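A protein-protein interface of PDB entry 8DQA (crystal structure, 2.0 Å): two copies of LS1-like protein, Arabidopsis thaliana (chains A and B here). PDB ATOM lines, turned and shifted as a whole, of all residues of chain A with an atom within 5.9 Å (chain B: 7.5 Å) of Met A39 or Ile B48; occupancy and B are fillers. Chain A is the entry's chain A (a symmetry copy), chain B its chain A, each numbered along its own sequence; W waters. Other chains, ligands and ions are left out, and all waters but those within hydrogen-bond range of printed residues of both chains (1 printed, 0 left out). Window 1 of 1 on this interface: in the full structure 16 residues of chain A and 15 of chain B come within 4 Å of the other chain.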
ATOM      1  N   PRO A   1     -14.258  -0.984  13.521  1.00  0.00           N
ATOM      2  CA  PRO A   1     -14.510  -0.359  12.217  1.00  0.00           C
ATOM      3  C   PRO A   1     -13.275  -0.329  11.323  1.00  0.00           C
ATOM      4  O   PRO A   1     -12.180  -0.043  11.807  1.00  0.00           O
ATOM      5  CB  PRO A   1     -14.941   1.060  12.597  1.00  0.00           C
ATOM      6  CG  PRO A   1     -14.214   1.333  13.864  1.00  0.00           C
ATOM      7  CD  PRO A   1     -14.133   0.014  14.598  1.00  0.00           C
ATOM      8  N   CYS A   2     -13.454  -0.622  10.036  1.00  0.00           N
ATOM      9  CA  CYS A   2     -12.361  -0.610   9.071  1.00  0.00           C
ATOM     10  C   CYS A   2     -12.638   0.448   8.013  1.00  0.00           C
ATOM     11  O   CYS A   2     -13.687   0.420   7.361  1.00  0.00           O
ATOM     12  CB  CYS A   2     -12.183  -1.974   8.406  1.00  0.00           C
ATOM     13  SG  CYS A   2     -10.926  -1.966   7.110  1.00  0.00           S
ATOM     14  N   LEU A   3     -11.692   1.366   7.836  1.00  0.00           N
ATOM     15  CA  LEU A   3     -11.760   2.395   6.802  1.00  0.00           C
ATOM     16  C   LEU A   3     -10.798   1.996   5.687  1.00  0.00           C
ATOM     17  O   LEU A   3      -9.579   2.004   5.875  1.00  0.00           O
ATOM     18  CB  LEU A   3     -11.418   3.763   7.385  1.00  0.00           C
ATOM     19  CG  LEU A   3     -11.292   4.934   6.410  1.00  0.00           C
ATOM     20  CD1 LEU A   3     -12.629   5.266   5.777  1.00  0.00           C
ATOM     21  CD2 LEU A   3     -10.719   6.153   7.125  1.00  0.00           C
ATOM     22  N   TYR A   4     -11.352   1.638   4.532  1.00  0.00           N
ATOM     23  CA  TYR A   4     -10.593   1.168   3.377  1.00  0.00           C
ATOM     24  C   TYR A   4     -10.576   2.276   2.335  1.00  0.00           C
ATOM     25  O   TYR A   4     -11.630   2.658   1.818  1.00  0.00           O
ATOM     26  CB  TYR A   4     -11.224  -0.108   2.817  1.00  0.00           C
ATOM     27  CG  TYR A   4     -10.359  -0.910   1.867  1.00  0.00           C
ATOM     28  CD1 TYR A   4     -10.139  -2.266   2.079  1.00  0.00           C
ATOM     29  CD2 TYR A   4      -9.789  -0.324   0.744  1.00  0.00           C
ATOM     30  CE1 TYR A   4      -9.364  -3.009   1.211  1.00  0.00           C
ATOM     31  CE2 TYR A   4      -9.010  -1.062  -0.129  1.00  0.00           C
ATOM     32  CZ  TYR A   4      -8.802  -2.403   0.109  1.00  0.00           C
ATOM     33  OH  TYR A   4      -8.029  -3.143  -0.754  1.00  0.00           O
ATOM     34  N   TYR A  20      -2.705   8.827   9.515  1.00  0.00           N
ATOM     35  CA  TYR A  20      -3.256   7.727  10.301  1.00  0.00           C
ATOM     36  C   TYR A  20      -3.610   8.186  11.709  1.00  0.00           C
ATOM     37  O   TYR A  20      -4.638   7.777  12.265  1.00  0.00           O
ATOM     38  CB  TYR A  20      -2.260   6.571  10.368  1.00  0.00           C
ATOM     39  CG  TYR A  20      -2.090   5.820   9.072  1.00  0.00           C
ATOM     40  CD1 TYR A  20      -3.176   5.243   8.430  1.00  0.00           C
ATOM     41  CD2 TYR A  20      -0.837   5.685   8.491  1.00  0.00           C
ATOM     42  CE1 TYR A  20      -3.020   4.559   7.243  1.00  0.00           C
ATOM     43  CE2 TYR A  20      -0.672   5.002   7.308  1.00  0.00           C
ATOM     44  CZ  TYR A  20      -1.766   4.442   6.688  1.00  0.00           C
ATOM     45  OH  TYR A  20      -1.598   3.760   5.508  1.00  0.00           O
ATOM     46  N   ASN A  36      -7.793   2.317  18.944  1.00  0.00           N
ATOM     47  CA  ASN A  36      -6.980   1.171  18.563  1.00  0.00           C
ATOM     48  C   ASN A  36      -7.752   0.119  17.782  1.00  0.00           C
ATOM     49  O   ASN A  36      -7.133  -0.791  17.220  1.00  0.00           O
ATOM     50  CB  ASN A  36      -6.374   0.513  19.804  1.00  0.00           C
ATOM     51  CG  ASN A  36      -4.920   0.869  19.997  1.00  0.00           C
ATOM     52  OD1 ASN A  36      -4.432   1.863  19.458  1.00  0.00           O
ATOM     53  ND2 ASN A  36      -4.214   0.056  20.776  1.00  0.00           N
ATOM     54  N   LEU A  37      -9.081   0.208  17.743  1.00  0.00           N
ATOM     55  CA  LEU A  37      -9.904  -0.751  17.022  1.00  0.00           C
ATOM     56  C   LEU A  37     -10.389  -0.209  15.684  1.00  0.00           C
ATOM     57  O   LEU A  37     -11.290  -0.796  15.074  1.00  0.00           O
ATOM     58  CB  LEU A  37     -11.092  -1.172  17.883  1.00  0.00           C
ATOM     59  CG  LEU A  37     -10.735  -1.835  19.214  1.00  0.00           C
ATOM     60  CD1 LEU A  37     -11.945  -2.580  19.766  1.00  0.00           C
ATOM     61  CD2 LEU A  37      -9.549  -2.778  19.086  1.00  0.00           C
ATOM     62  N   VAL A  38      -9.819   0.897  15.219  1.00  0.00           N
ATOM     63  CA  VAL A  38     -10.085   1.428  13.888  1.00  0.00           C
ATOM     64  C   VAL A  38      -8.971   0.917  12.984  1.00  0.00           C
ATOM     65  O   VAL A  38      -7.800   1.272  13.166  1.00  0.00           O
ATOM     66  CB  VAL A  38     -10.152   2.961  13.893  1.00  0.00           C
ATOM     67  CG1 VAL A  38     -10.206   3.509  12.470  1.00  0.00           C
ATOM     68  CG2 VAL A  38     -11.361   3.438  14.692  1.00  0.00           C
ATOM     69  N   MET A  39      -9.321   0.062  12.026  1.00  0.00           N
ATOM     70  CA  MET A  39      -8.383  -0.367  10.998  1.00  0.00           C
ATOM     71  C   MET A  39      -8.457   0.610   9.831  1.00  0.00           C
ATOM     72  O   MET A  39      -9.553   0.974   9.388  1.00  0.00           O
ATOM     73  CB  MET A  39      -8.686  -1.785  10.513  1.00  0.00           C
ATOM     74  CG  MET A  39      -7.580  -2.364   9.632  1.00  0.00           C
ATOM     75  SD  MET A  39      -8.003  -3.886   8.758  1.00  0.00           S
ATOM     76  CE  MET A  39      -7.513  -5.112   9.965  1.00  0.00           C
ATOM     77  N   VAL A  40      -7.296   1.039   9.343  1.00  0.00           N
ATOM     78  CA  VAL A  40      -7.201   1.888   8.162  1.00  0.00           C
ATOM     79  C   VAL A  40      -6.392   1.147   7.107  1.00  0.00           C
ATOM     80  O   VAL A  40      -5.263   0.716   7.372  1.00  0.00           O
ATOM     81  CB  VAL A  40      -6.559   3.252   8.477  1.00  0.00           C
ATOM     82  CG1 VAL A  40      -6.563   4.135   7.233  1.00  0.00           C
ATOM     83  CG2 VAL A  40      -7.292   3.933   9.621  1.00  0.00           C
ATOM     84  N   VAL A  41      -6.974   0.995   5.920  1.00  0.00           N
ATOM     85  CA  VAL A  41      -6.304   0.406   4.766  1.00  0.00           C
ATOM     86  C   VAL A  41      -6.170   1.497   3.715  1.00  0.00           C
ATOM     87  O   VAL A  41      -7.177   1.991   3.192  1.00  0.00           O
ATOM     88  CB  VAL A  41      -7.075  -0.801   4.213  1.00  0.00           C
ATOM     89  CG1 VAL A  41      -6.272  -1.482   3.120  1.00  0.00           C
ATOM     90  CG2 VAL A  41      -7.403  -1.773   5.332  1.00  0.00           C
ATOM     91  N   LEU A  42      -4.933   1.869   3.401  1.00  0.00           N
ATOM     92  CA  LEU A  42      -4.649   2.985   2.503  1.00  0.00           C
ATOM     93  C   LEU A  42      -3.860   2.464   1.310  1.00  0.00           C
ATOM     94  O   LEU A  42      -2.680   2.120   1.441  1.00  0.00           O
ATOM     95  CB  LEU A  42      -3.882   4.083   3.236  1.00  0.00           C
ATOM     96  CG  LEU A  42      -3.543   5.339   2.436  1.00  0.00           C
ATOM     97  CD1 LEU A  42      -4.806   6.053   1.989  1.00  0.00           C
ATOM     98  CD2 LEU A  42      -2.662   6.268   3.263  1.00  0.00           C
ATOM     99  N   THR B   6      -7.147  -8.268   1.354  1.00  0.00           N
ATOM    100  CA  THR B   6      -6.172  -7.185   1.319  1.00  0.00           C
ATOM    101  C   THR B   6      -5.341  -7.242   2.595  1.00  0.00           C
ATOM    102  O   THR B   6      -5.896  -7.282   3.699  1.00  0.00           O
ATOM    103  CB  THR B   6      -6.864  -5.826   1.198  1.00  0.00           C
ATOM    104  OG1 THR B   6      -7.645  -5.789  -0.004  1.00  0.00           O
ATOM    105  CG2 THR B   6      -5.842  -4.710   1.164  1.00  0.00           C
ATOM    106  N   THR B   7      -4.017  -7.244   2.445  1.00  0.00           N
ATOM    107  CA  THR B   7      -3.131  -7.398   3.590  1.00  0.00           C
ATOM    108  C   THR B   7      -1.861  -6.591   3.367  1.00  0.00           C
ATOM    109  O   THR B   7      -1.472  -6.302   2.234  1.00  0.00           O
ATOM    110  CB  THR B   7      -2.775  -8.872   3.834  1.00  0.00           C
ATOM    111  OG1 THR B   7      -1.720  -8.959   4.801  1.00  0.00           O
ATOM    112  CG2 THR B   7      -2.322  -9.537   2.539  1.00  0.00           C
ATOM    113  N   ASN B   8      -1.211  -6.231   4.476  1.00  0.00           N
ATOM    114  CA  ASN B   8       0.075  -5.546   4.423  1.00  0.00           C
ATOM    115  C   ASN B   8       1.245  -6.512   4.280  1.00  0.00           C
ATOM    116  O   ASN B   8       2.389  -6.061   4.160  1.00  0.00           O
ATOM    117  CB  ASN B   8       0.271  -4.684   5.673  1.00  0.00           C
ATOM    118  CG  ASN B   8       0.047  -5.454   6.961  1.00  0.00           C
ATOM    119  OD1 ASN B   8      -0.285  -6.640   6.947  1.00  0.00           O
ATOM    120  ND2 ASN B   8       0.228  -4.776   8.088  1.00  0.00           N
ATOM    121  N   VAL B   9       0.987  -7.820   4.292  1.00  0.00           N
ATOM    122  CA  VAL B   9       2.043  -8.802   4.092  1.00  0.00           C
ATOM    123  C   VAL B   9       2.579  -8.691   2.672  1.00  0.00           C
ATOM    124  O   VAL B   9       1.825  -8.466   1.716  1.00  0.00           O
ATOM    125  CB  VAL B   9       1.506 -10.213   4.387  1.00  0.00           C
ATOM    126  CG1 VAL B   9       2.435 -11.272   3.829  1.00  0.00           C
ATOM    127  CG2 VAL B   9       1.307 -10.400   5.887  1.00  0.00           C
ATOM    128  N   LYS B  43      -4.400  -9.390  -2.471  1.00  0.00           N
ATOM    129  CA  LYS B  43      -3.634  -8.175  -2.725  1.00  0.00           C
ATOM    130  C   LYS B  43      -2.758  -7.891  -1.513  1.00  0.00           C
ATOM    131  O   LYS B  43      -3.262  -7.508  -0.451  1.00  0.00           O
ATOM    132  CB  LYS B  43      -4.557  -6.994  -3.017  1.00  0.00           C
ATOM    133  CG  LYS B  43      -3.823  -5.673  -3.239  1.00  0.00           C
ATOM    134  CD  LYS B  43      -2.607  -5.856  -4.144  1.00  0.00           C
ATOM    135  CE  LYS B  43      -2.091  -4.531  -4.686  1.00  0.00           C
ATOM    136  NZ  LYS B  43      -1.519  -4.682  -6.057  1.00  0.00           N
ATOM    137  N   SER B  45       1.064  -6.166   0.177  1.00  0.00           N
ATOM    138  CA  SER B  45       1.862  -4.941   0.171  1.00  0.00           C
ATOM    139  C   SER B  45       0.986  -3.691   0.179  1.00  0.00           C
ATOM    140  O   SER B  45       1.310  -2.681  -0.443  1.00  0.00           O
ATOM    141  CB  SER B  45       2.812  -4.913  -1.030  1.00  0.00           C
ATOM    142  OG  SER B  45       3.608  -6.079  -1.077  1.00  0.00           O
ATOM    143  N   VAL B  46      -0.135  -3.759   0.893  1.00  0.00           N
ATOM    144  CA  VAL B  46      -1.018  -2.612   1.092  1.00  0.00           C
ATOM    145  C   VAL B  46      -0.859  -2.163   2.536  1.00  0.00           C
ATOM    146  O   VAL B  46      -0.987  -2.975   3.460  1.00  0.00           O
ATOM    147  CB  VAL B  46      -2.483  -2.959   0.776  1.00  0.00           C
ATOM    148  CG1 VAL B  46      -3.407  -1.825   1.195  1.00  0.00           C
ATOM    149  CG2 VAL B  46      -2.650  -3.256  -0.707  1.00  0.00           C
ATOM    150  N   GLU B  47      -0.568  -0.882   2.735  1.00  0.00           N
ATOM    151  CA  GLU B  47      -0.317  -0.391   4.081  1.00  0.00           C
ATOM    152  C   GLU B  47      -1.593  -0.464   4.911  1.00  0.00           C
ATOM    153  O   GLU B  47      -2.661  -0.021   4.472  1.00  0.00           O
ATOM    154  CB  GLU B  47       0.214   1.040   4.043  1.00  0.00           C
ATOM    155  CG  GLU B  47       0.784   1.503   5.377  1.00  0.00           C
ATOM    156  CD  GLU B  47       1.670   2.727   5.251  1.00  0.00           C
ATOM    157  OE1 GLU B  47       1.171   3.783   4.804  1.00  0.00           O
ATOM    158  OE2 GLU B  47       2.866   2.634   5.605  1.00  0.00           O
ATOM    159  N   ILE B  48      -1.477  -1.034   6.110  1.00  0.00           N
ATOM    160  CA  ILE B  48      -2.586  -1.154   7.046  1.00  0.00           C
ATOM    161  C   ILE B  48      -2.112  -0.680   8.411  1.00  0.00           C
ATOM    162  O   ILE B  48      -0.947  -0.855   8.781  1.00  0.00           O
ATOM    163  CB  ILE B  48      -3.126  -2.602   7.130  1.00  0.00           C
ATOM    164  CG1 ILE B  48      -3.582  -3.071   5.745  1.00  0.00           C
ATOM    165  CG2 ILE B  48      -4.255  -2.685   8.148  1.00  0.00           C
ATOM    166  CD1 ILE B  48      -4.231  -4.442   5.726  1.00  0.00           C
ATOM    167  N   VAL B  49      -3.028  -0.075   9.162  1.00  0.00           N
ATOM    168  CA  VAL B  49      -2.787   0.341  10.539  1.00  0.00           C
ATOM    169  C   VAL B  49      -3.931  -0.193  11.389  1.00  0.00           C
ATOM    170  O   VAL B  49      -5.104   0.019  11.062  1.00  0.00           O
ATOM    171  CB  VAL B  49      -2.675   1.872  10.664  1.00  0.00           C
ATOM    172  CG1 VAL B  49      -2.969   2.315  12.092  1.00  0.00           C
ATOM    173  CG2 VAL B  49      -1.290   2.343  10.224  1.00  0.00           C
ATOM    174  N   PHE B  50      -3.593  -0.890  12.471  1.00  0.00           N
ATOM    175  CA  PHE B  50      -4.595  -1.471  13.351  1.00  0.00           C
ATOM    176  C   PHE B  50      -3.947  -1.753  14.698  1.00  0.00           C
ATOM    177  O   PHE B  50      -2.799  -2.202  14.758  1.00  0.00           O
ATOM    178  CB  PHE B  50      -5.182  -2.754  12.756  1.00  0.00           C
ATOM    179  CG  PHE B  50      -6.365  -3.289  13.512  1.00  0.00           C
ATOM    180  CD1 PHE B  50      -6.375  -4.597  13.966  1.00  0.00           C
ATOM    181  CD2 PHE B  50      -7.470  -2.491  13.760  1.00  0.00           C
ATOM    182  CE1 PHE B  50      -7.462  -5.098  14.656  1.00  0.00           C
ATOM    183  CE2 PHE B  50      -8.559  -2.985  14.450  1.00  0.00           C
ATOM    184  CZ  PHE B  50      -8.555  -4.290  14.898  1.00  0.00           C
ATOM    185  N   GLY B  51      -4.689  -1.493  15.770  1.00  0.00           N
ATOM    186  CA  GLY B  51      -4.111  -1.594  17.093  1.00  0.00           C
ATOM    187  C   GLY B  51      -2.994  -0.612  17.339  1.00  0.00           C
ATOM    188  O   GLY B  51      -2.173  -0.826  18.235  1.00  0.00           O
ATOM    189  N   ASN B  53      -0.466   0.001  15.353  1.00  0.00           N
ATOM    190  CA  ASN B  53       0.792  -0.403  14.750  1.00  0.00           C
ATOM    191  C   ASN B  53       0.520  -0.987  13.373  1.00  0.00           C
ATOM    192  O   ASN B  53      -0.630  -1.087  12.928  1.00  0.00           O
ATOM    193  CB  ASN B  53       1.543  -1.398  15.649  1.00  0.00           C
ATOM    194  CG  ASN B  53       0.763  -2.673  15.897  1.00  0.00           C
ATOM    195  OD1 ASN B  53       0.130  -3.215  14.993  1.00  0.00           O
ATOM    196  ND2 ASN B  53       0.815  -3.167  17.130  1.00  0.00           N
ATOM    197  N   LYS B  54       1.596  -1.371  12.686  1.00  0.00           N
ATOM    198  CA  LYS B  54       1.522  -1.890  11.328  1.00  0.00           C
ATOM    199  C   LYS B  54       1.923  -3.360  11.259  1.00  0.00           C
ATOM    200  O   LYS B  54       2.439  -3.821  10.238  1.00  0.00           O
ATOM    201  CB  LYS B  54       2.402  -1.057  10.395  1.00  0.00           C
ATOM    202  CG  LYS B  54       2.127   0.440  10.454  1.00  0.00           C
ATOM    203  CD  LYS B  54       3.006   1.214   9.478  1.00  0.00           C
ATOM    204  CE  LYS B  54       2.406   2.573   9.150  1.00  0.00           C
ATOM    205  NZ  LYS B  54       2.568   3.540  10.272  1.00  0.00           N
ATOM    206  N   GLU B  55       1.697  -4.104  12.337  1.00  0.00           N
ATOM    207  CA  GLU B  55       1.932  -5.539  12.304  1.00  0.00           C
ATOM    208  C   GLU B  55       1.070  -6.182  11.220  1.00  0.00           C
ATOM    209  O   GLU B  55       0.105  -5.593  10.722  1.00  0.00           O
ATOM    210  CB  GLU B  55       1.627  -6.161  13.664  1.00  0.00           C
ATOM    211  CG  GLU B  55       2.676  -5.875  14.727  1.00  0.00           C
ATOM    212  CD  GLU B  55       2.447  -6.676  15.993  1.00  0.00           C
ATOM    213  OE1 GLU B  55       2.719  -7.895  15.979  1.00  0.00           O
ATOM    214  OE2 GLU B  55       1.988  -6.086  16.996  1.00  0.00           O
ATOM    215  N   ALA B  56       1.434  -7.408  10.847  1.00  0.00           N
ATOM    216  CA  ALA B  56       0.678  -8.142   9.841  1.00  0.00           C
ATOM    217  C   ALA B  56      -0.811  -8.101  10.162  1.00  0.00           C
ATOM    218  O   ALA B  56      -1.231  -8.406  11.280  1.00  0.00           O
ATOM    219  CB  ALA B  56       1.169  -9.588   9.768  1.00  0.00           C
ATOM    220  N   ALA B  57      -1.605  -7.702   9.170  1.00  0.00           N
ATOM    221  CA  ALA B  57      -3.045  -7.577   9.330  1.00  0.00           C
ATOM    222  C   ALA B  57      -3.695  -7.769   7.970  1.00  0.00           C
ATOM    223  O   ALA B  57      -3.033  -7.708   6.929  1.00  0.00           O
ATOM    224  CB  ALA B  57      -3.432  -6.221   9.928  1.00  0.00           C
ATOM    225  N   ALA B  58      -5.006  -8.002   7.986  1.00  0.00           N
ATOM    226  CA  ALA B  58      -5.738  -8.228   6.751  1.00  0.00           C
ATOM    227  C   ALA B  58      -7.187  -7.799   6.914  1.00  0.00           C
ATOM    228  O   ALA B  58      -7.771  -7.915   7.995  1.00  0.00           O
ATOM    229  CB  ALA B  58      -5.682  -9.703   6.327  1.00  0.00           C
ATOM    230  N   TYR B  59      -7.749  -7.286   5.823  1.00  0.00           N
ATOM    231  CA  TYR B  59      -9.181  -7.075   5.685  1.00  0.00           C
ATOM    232  C   TYR B  59      -9.658  -7.941   4.529  1.00  0.00           C
ATOM    233  O   TYR B  59      -9.020  -7.970   3.471  1.00  0.00           O
ATOM    234  CB  TYR B  59      -9.524  -5.615   5.423  1.00  0.00           C
ATOM    235  CG  TYR B  59     -10.972  -5.391   5.059  1.00  0.00           C
ATOM    236  CD1 TYR B  59     -11.344  -5.107   3.754  1.00  0.00           C
ATOM    237  CD2 TYR B  59     -11.975  -5.492   6.018  1.00  0.00           C
ATOM    238  CE1 TYR B  59     -12.670  -4.915   3.414  1.00  0.00           C
ATOM    239  CE2 TYR B  59     -13.299  -5.301   5.687  1.00  0.00           C
ATOM    240  CZ  TYR B  59     -13.642  -5.012   4.386  1.00  0.00           C
ATOM    241  OH  TYR B  59     -14.961  -4.823   4.051  1.00  0.00           O
ATOM    242  N   ALA B  60     -10.758  -8.655   4.737  1.00  0.00           N
ATOM    243  CA  ALA B  60     -11.309  -9.528   3.716  1.00  0.00           C
ATOM    244  C   ALA B  60     -12.812  -9.326   3.616  1.00  0.00           C
ATOM    245  O   ALA B  60     -13.481  -8.974   4.591  1.00  0.00           O
ATOM    246  CB  ALA B  60     -11.012 -11.007   4.004  1.00  0.00           C
ATOM    247  N   THR B  93      -6.530 -12.005  15.457  1.00  0.00           N
ATOM    248  CA  THR B  93      -6.937 -10.788  16.148  1.00  0.00           C
ATOM    249  C   THR B  93      -6.754  -9.555  15.278  1.00  0.00           C
ATOM    250  O   THR B  93      -7.310  -8.497  15.595  1.00  0.00           O
ATOM    251  CB  THR B  93      -6.145 -10.609  17.443  1.00  0.00           C
ATOM    252  OG1 THR B  93      -4.749 -10.788  17.179  1.00  0.00           O
ATOM    253  CG2 THR B  93      -6.605 -11.610  18.493  1.00  0.00           C
ATOM    254  N   ARG B  94      -5.979  -9.664  14.201  1.00  0.00           N
ATOM    255  CA  ARG B  94      -5.743  -8.569  13.268  1.00  0.00           C
ATOM    256  C   ARG B  94      -6.357  -8.861  11.902  1.00  0.00           C
ATOM    257  O   ARG B  94      -5.881  -8.366  10.878  1.00  0.00           O
ATOM    258  CB  ARG B  94      -4.244  -8.296  13.150  1.00  0.00           C
ATOM    259  CG  ARG B  94      -3.616  -7.830  14.457  1.00  0.00           C
ATOM    260  CD  ARG B  94      -2.116  -7.643  14.331  1.00  0.00           C
ATOM    261  NE  ARG B  94      -1.767  -6.540  13.440  1.00  0.00           N
ATOM    262  CZ  ARG B  94      -1.915  -5.255  13.743  1.00  0.00           C
ATOM    263  NH1 ARG B  94      -2.409  -4.897  14.920  1.00  0.00           N
ATOM    264  NH2 ARG B  94      -1.566  -4.324  12.866  1.00  0.00           N
ATOM    265  N   PHE B  95      -7.421  -9.660  11.883  1.00  0.00           N
ATOM    266  CA  PHE B  95      -8.120 -10.056  10.665  1.00  0.00           C
ATOM    267  C   PHE B  95      -9.562  -9.580  10.782  1.00  0.00           C
ATOM    268  O   PHE B  95     -10.304 -10.048  11.653  1.00  0.00           O
ATOM    269  CB  PHE B  95      -8.044 -11.570  10.474  1.00  0.00           C
ATOM    270  CG  PHE B  95      -8.748 -12.070   9.246  1.00  0.00           C
ATOM    271  CD1 PHE B  95      -8.605 -11.419   8.031  1.00  0.00           C
ATOM    272  CD2 PHE B  95      -9.548 -13.198   9.305  1.00  0.00           C
ATOM    273  CE1 PHE B  95      -9.253 -11.881   6.899  1.00  0.00           C
ATOM    274  CE2 PHE B  95     -10.197 -13.664   8.179  1.00  0.00           C
ATOM    275  CZ  PHE B  95     -10.050 -13.006   6.975  1.00  0.00           C
ATOM    276  N   ILE B  96      -9.952  -8.643   9.920  1.00  0.00           N
ATOM    277  CA  ILE B  96     -11.324  -8.143   9.849  1.00  0.00           C
ATOM    278  C   ILE B  96     -11.961  -8.734   8.596  1.00  0.00           C
ATOM    279  O   ILE B  96     -11.445  -8.558   7.485  1.00  0.00           O
ATOM    280  CB  ILE B  96     -11.380  -6.610   9.834  1.00  0.00           C
ATOM    281  CG1 ILE B  96     -10.892  -6.064  11.178  1.00  0.00           C
ATOM    282  CG2 ILE B  96     -12.793  -6.137   9.535  1.00  0.00           C
ATOM    283  CD1 ILE B  96     -10.988  -4.557  11.325  1.00  0.00           C
ATOM    284  N   PHE B  97     -13.094  -9.416   8.769  1.00  0.00           N
ATOM    285  CA  PHE B  97     -13.716 -10.200   7.704  1.00  0.00           C
ATOM    286  C   PHE B  97     -15.186  -9.826   7.583  1.00  0.00           C
ATOM    287  O   PHE B  97     -15.999 -10.206   8.432  1.00  0.00           O
ATOM    288  CB  PHE B  97     -13.558 -11.696   7.989  1.00  0.00           C
ATOM    289  CG  PHE B  97     -13.826 -12.585   6.805  1.00  0.00           C
ATOM    290  CD1 PHE B  97     -14.207 -12.062   5.581  1.00  0.00           C
ATOM    291  CD2 PHE B  97     -13.692 -13.957   6.926  1.00  0.00           C
ATOM    292  CE1 PHE B  97     -14.450 -12.892   4.502  1.00  0.00           C
ATOM    293  CE2 PHE B  97     -13.931 -14.789   5.852  1.00  0.00           C
ATOM    294  CZ  PHE B  97     -14.313 -14.257   4.640  1.00  0.00           C
HETATM  295  O   HOH W   1      -0.129   1.180   0.600  1.00  0.00           O
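Of the 12 printed residues of chain A, 10 touch a printed residue of chain B.
Hydrophobic or aromatic side chains of chain A within 4 Å of the printed part of chain B: Tyr A4, Tyr A20, Met A39 and Val A41.
Of the 25 printed residues of chain B, 11 touch a printed residue of chain A.
Hydrophobic or aromatic side chains of chain B within 4 Å of the printed part of chain A: Val B46, Ile B48, Val B49, Phe B50, Tyr B59 and Ile B96.
Among the printed residues, no Asp or Glu carboxylate lies within 4 Å of a Lys or Arg side-chain nitrogen of the other chain.
Water W1 bridges O of Leu A42 and N of Glu B47.
The backbone carbonyl oxygen (O) of Thr B6 is in hydrogen-bond range of the backbone NH (N) of Tyr B59, at 2.8 Å.
The side-chain amide oxygen (OD1) of Asn B53 sits close to the backbone carbonyl oxygen (O) of Phe B50, at 3.1 Å.
The backbone carbonyl oxygen of Phe B50 lies within hydrogen-bond range of the guanidinium group of Arg B94 (2.7 Å).
O of Glu B55 sits at hydrogen-bond distance from NH2 of Arg B94 (3.0 Å).
The backbone carbonyl oxygen (O) of Met A39 lies within hydrogen-bond range of the backbone NH (N) of Leu A3 (2.7 Å).
The backbone NH (N) of Val A41 is in hydrogen-bond range of the backbone carbonyl oxygen (O) of Leu A3 (2.8 Å).
Among the printed residues, pairs that only touch across the chains: Val A40 with Ile B48, Met A39 with Val B49, Met A39 with Ala B58, Val A41 with Val B46, Tyr A4 with Tyr B59, Met A39 with Phe B50, Leu A37 with Phe B50, Val A38 with Val B49, Met A39 with Ile B48, Val A41 with Glu B47, Met A39 with Ile B96, Tyr A20 with Val B49, Met A39 with Arg B94, Val A41 with Thr B6, Val A38 with Phe B50, Asn A36 with Phe B50, Cys A2 with Tyr B59 and Val A40 with Glu B47.
Of the printed residues of chain B, Met A39 touches Ile B48 (3.7 Å), Val B49 (3.3 Å), Phe B50 (3.5 Å), Ala B58 (3.4 Å), Arg B94 (3.8 Å) and Ile B96 (3.7 Å).
Of chain A, only Met A39 (3.7 Å) and Val A40 (3.3 Å) come within 4 Å of Ile B48.
Of the printed residues of chain B, Cys A2 touches Tyr B59 (3.8 Å).
Of the printed residues of chain A, Ala B58 touches Met A39.
No position is printed for both chains.
OG1 of Thr B6 sits at hydrogen-bond distance from OH of Tyr A4.
The side-chain carboxylate (OE1) of Glu B47 sits at hydrogen-bond distance from the side-chain hydroxyl (OH) of Tyr A20, 2.9 Å away.
O of Glu B47 is in hydrogen-bond range of N of Leu A42, at 3.1 Å.
The backbone NH (N) of Val A40 sits at hydrogen-bond distance from the backbone carbonyl oxygen (O) of Val B49 (3.0 Å).
O of Asn A36 is in hydrogen-bond range of N of Gly B51 (2.9 Å).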
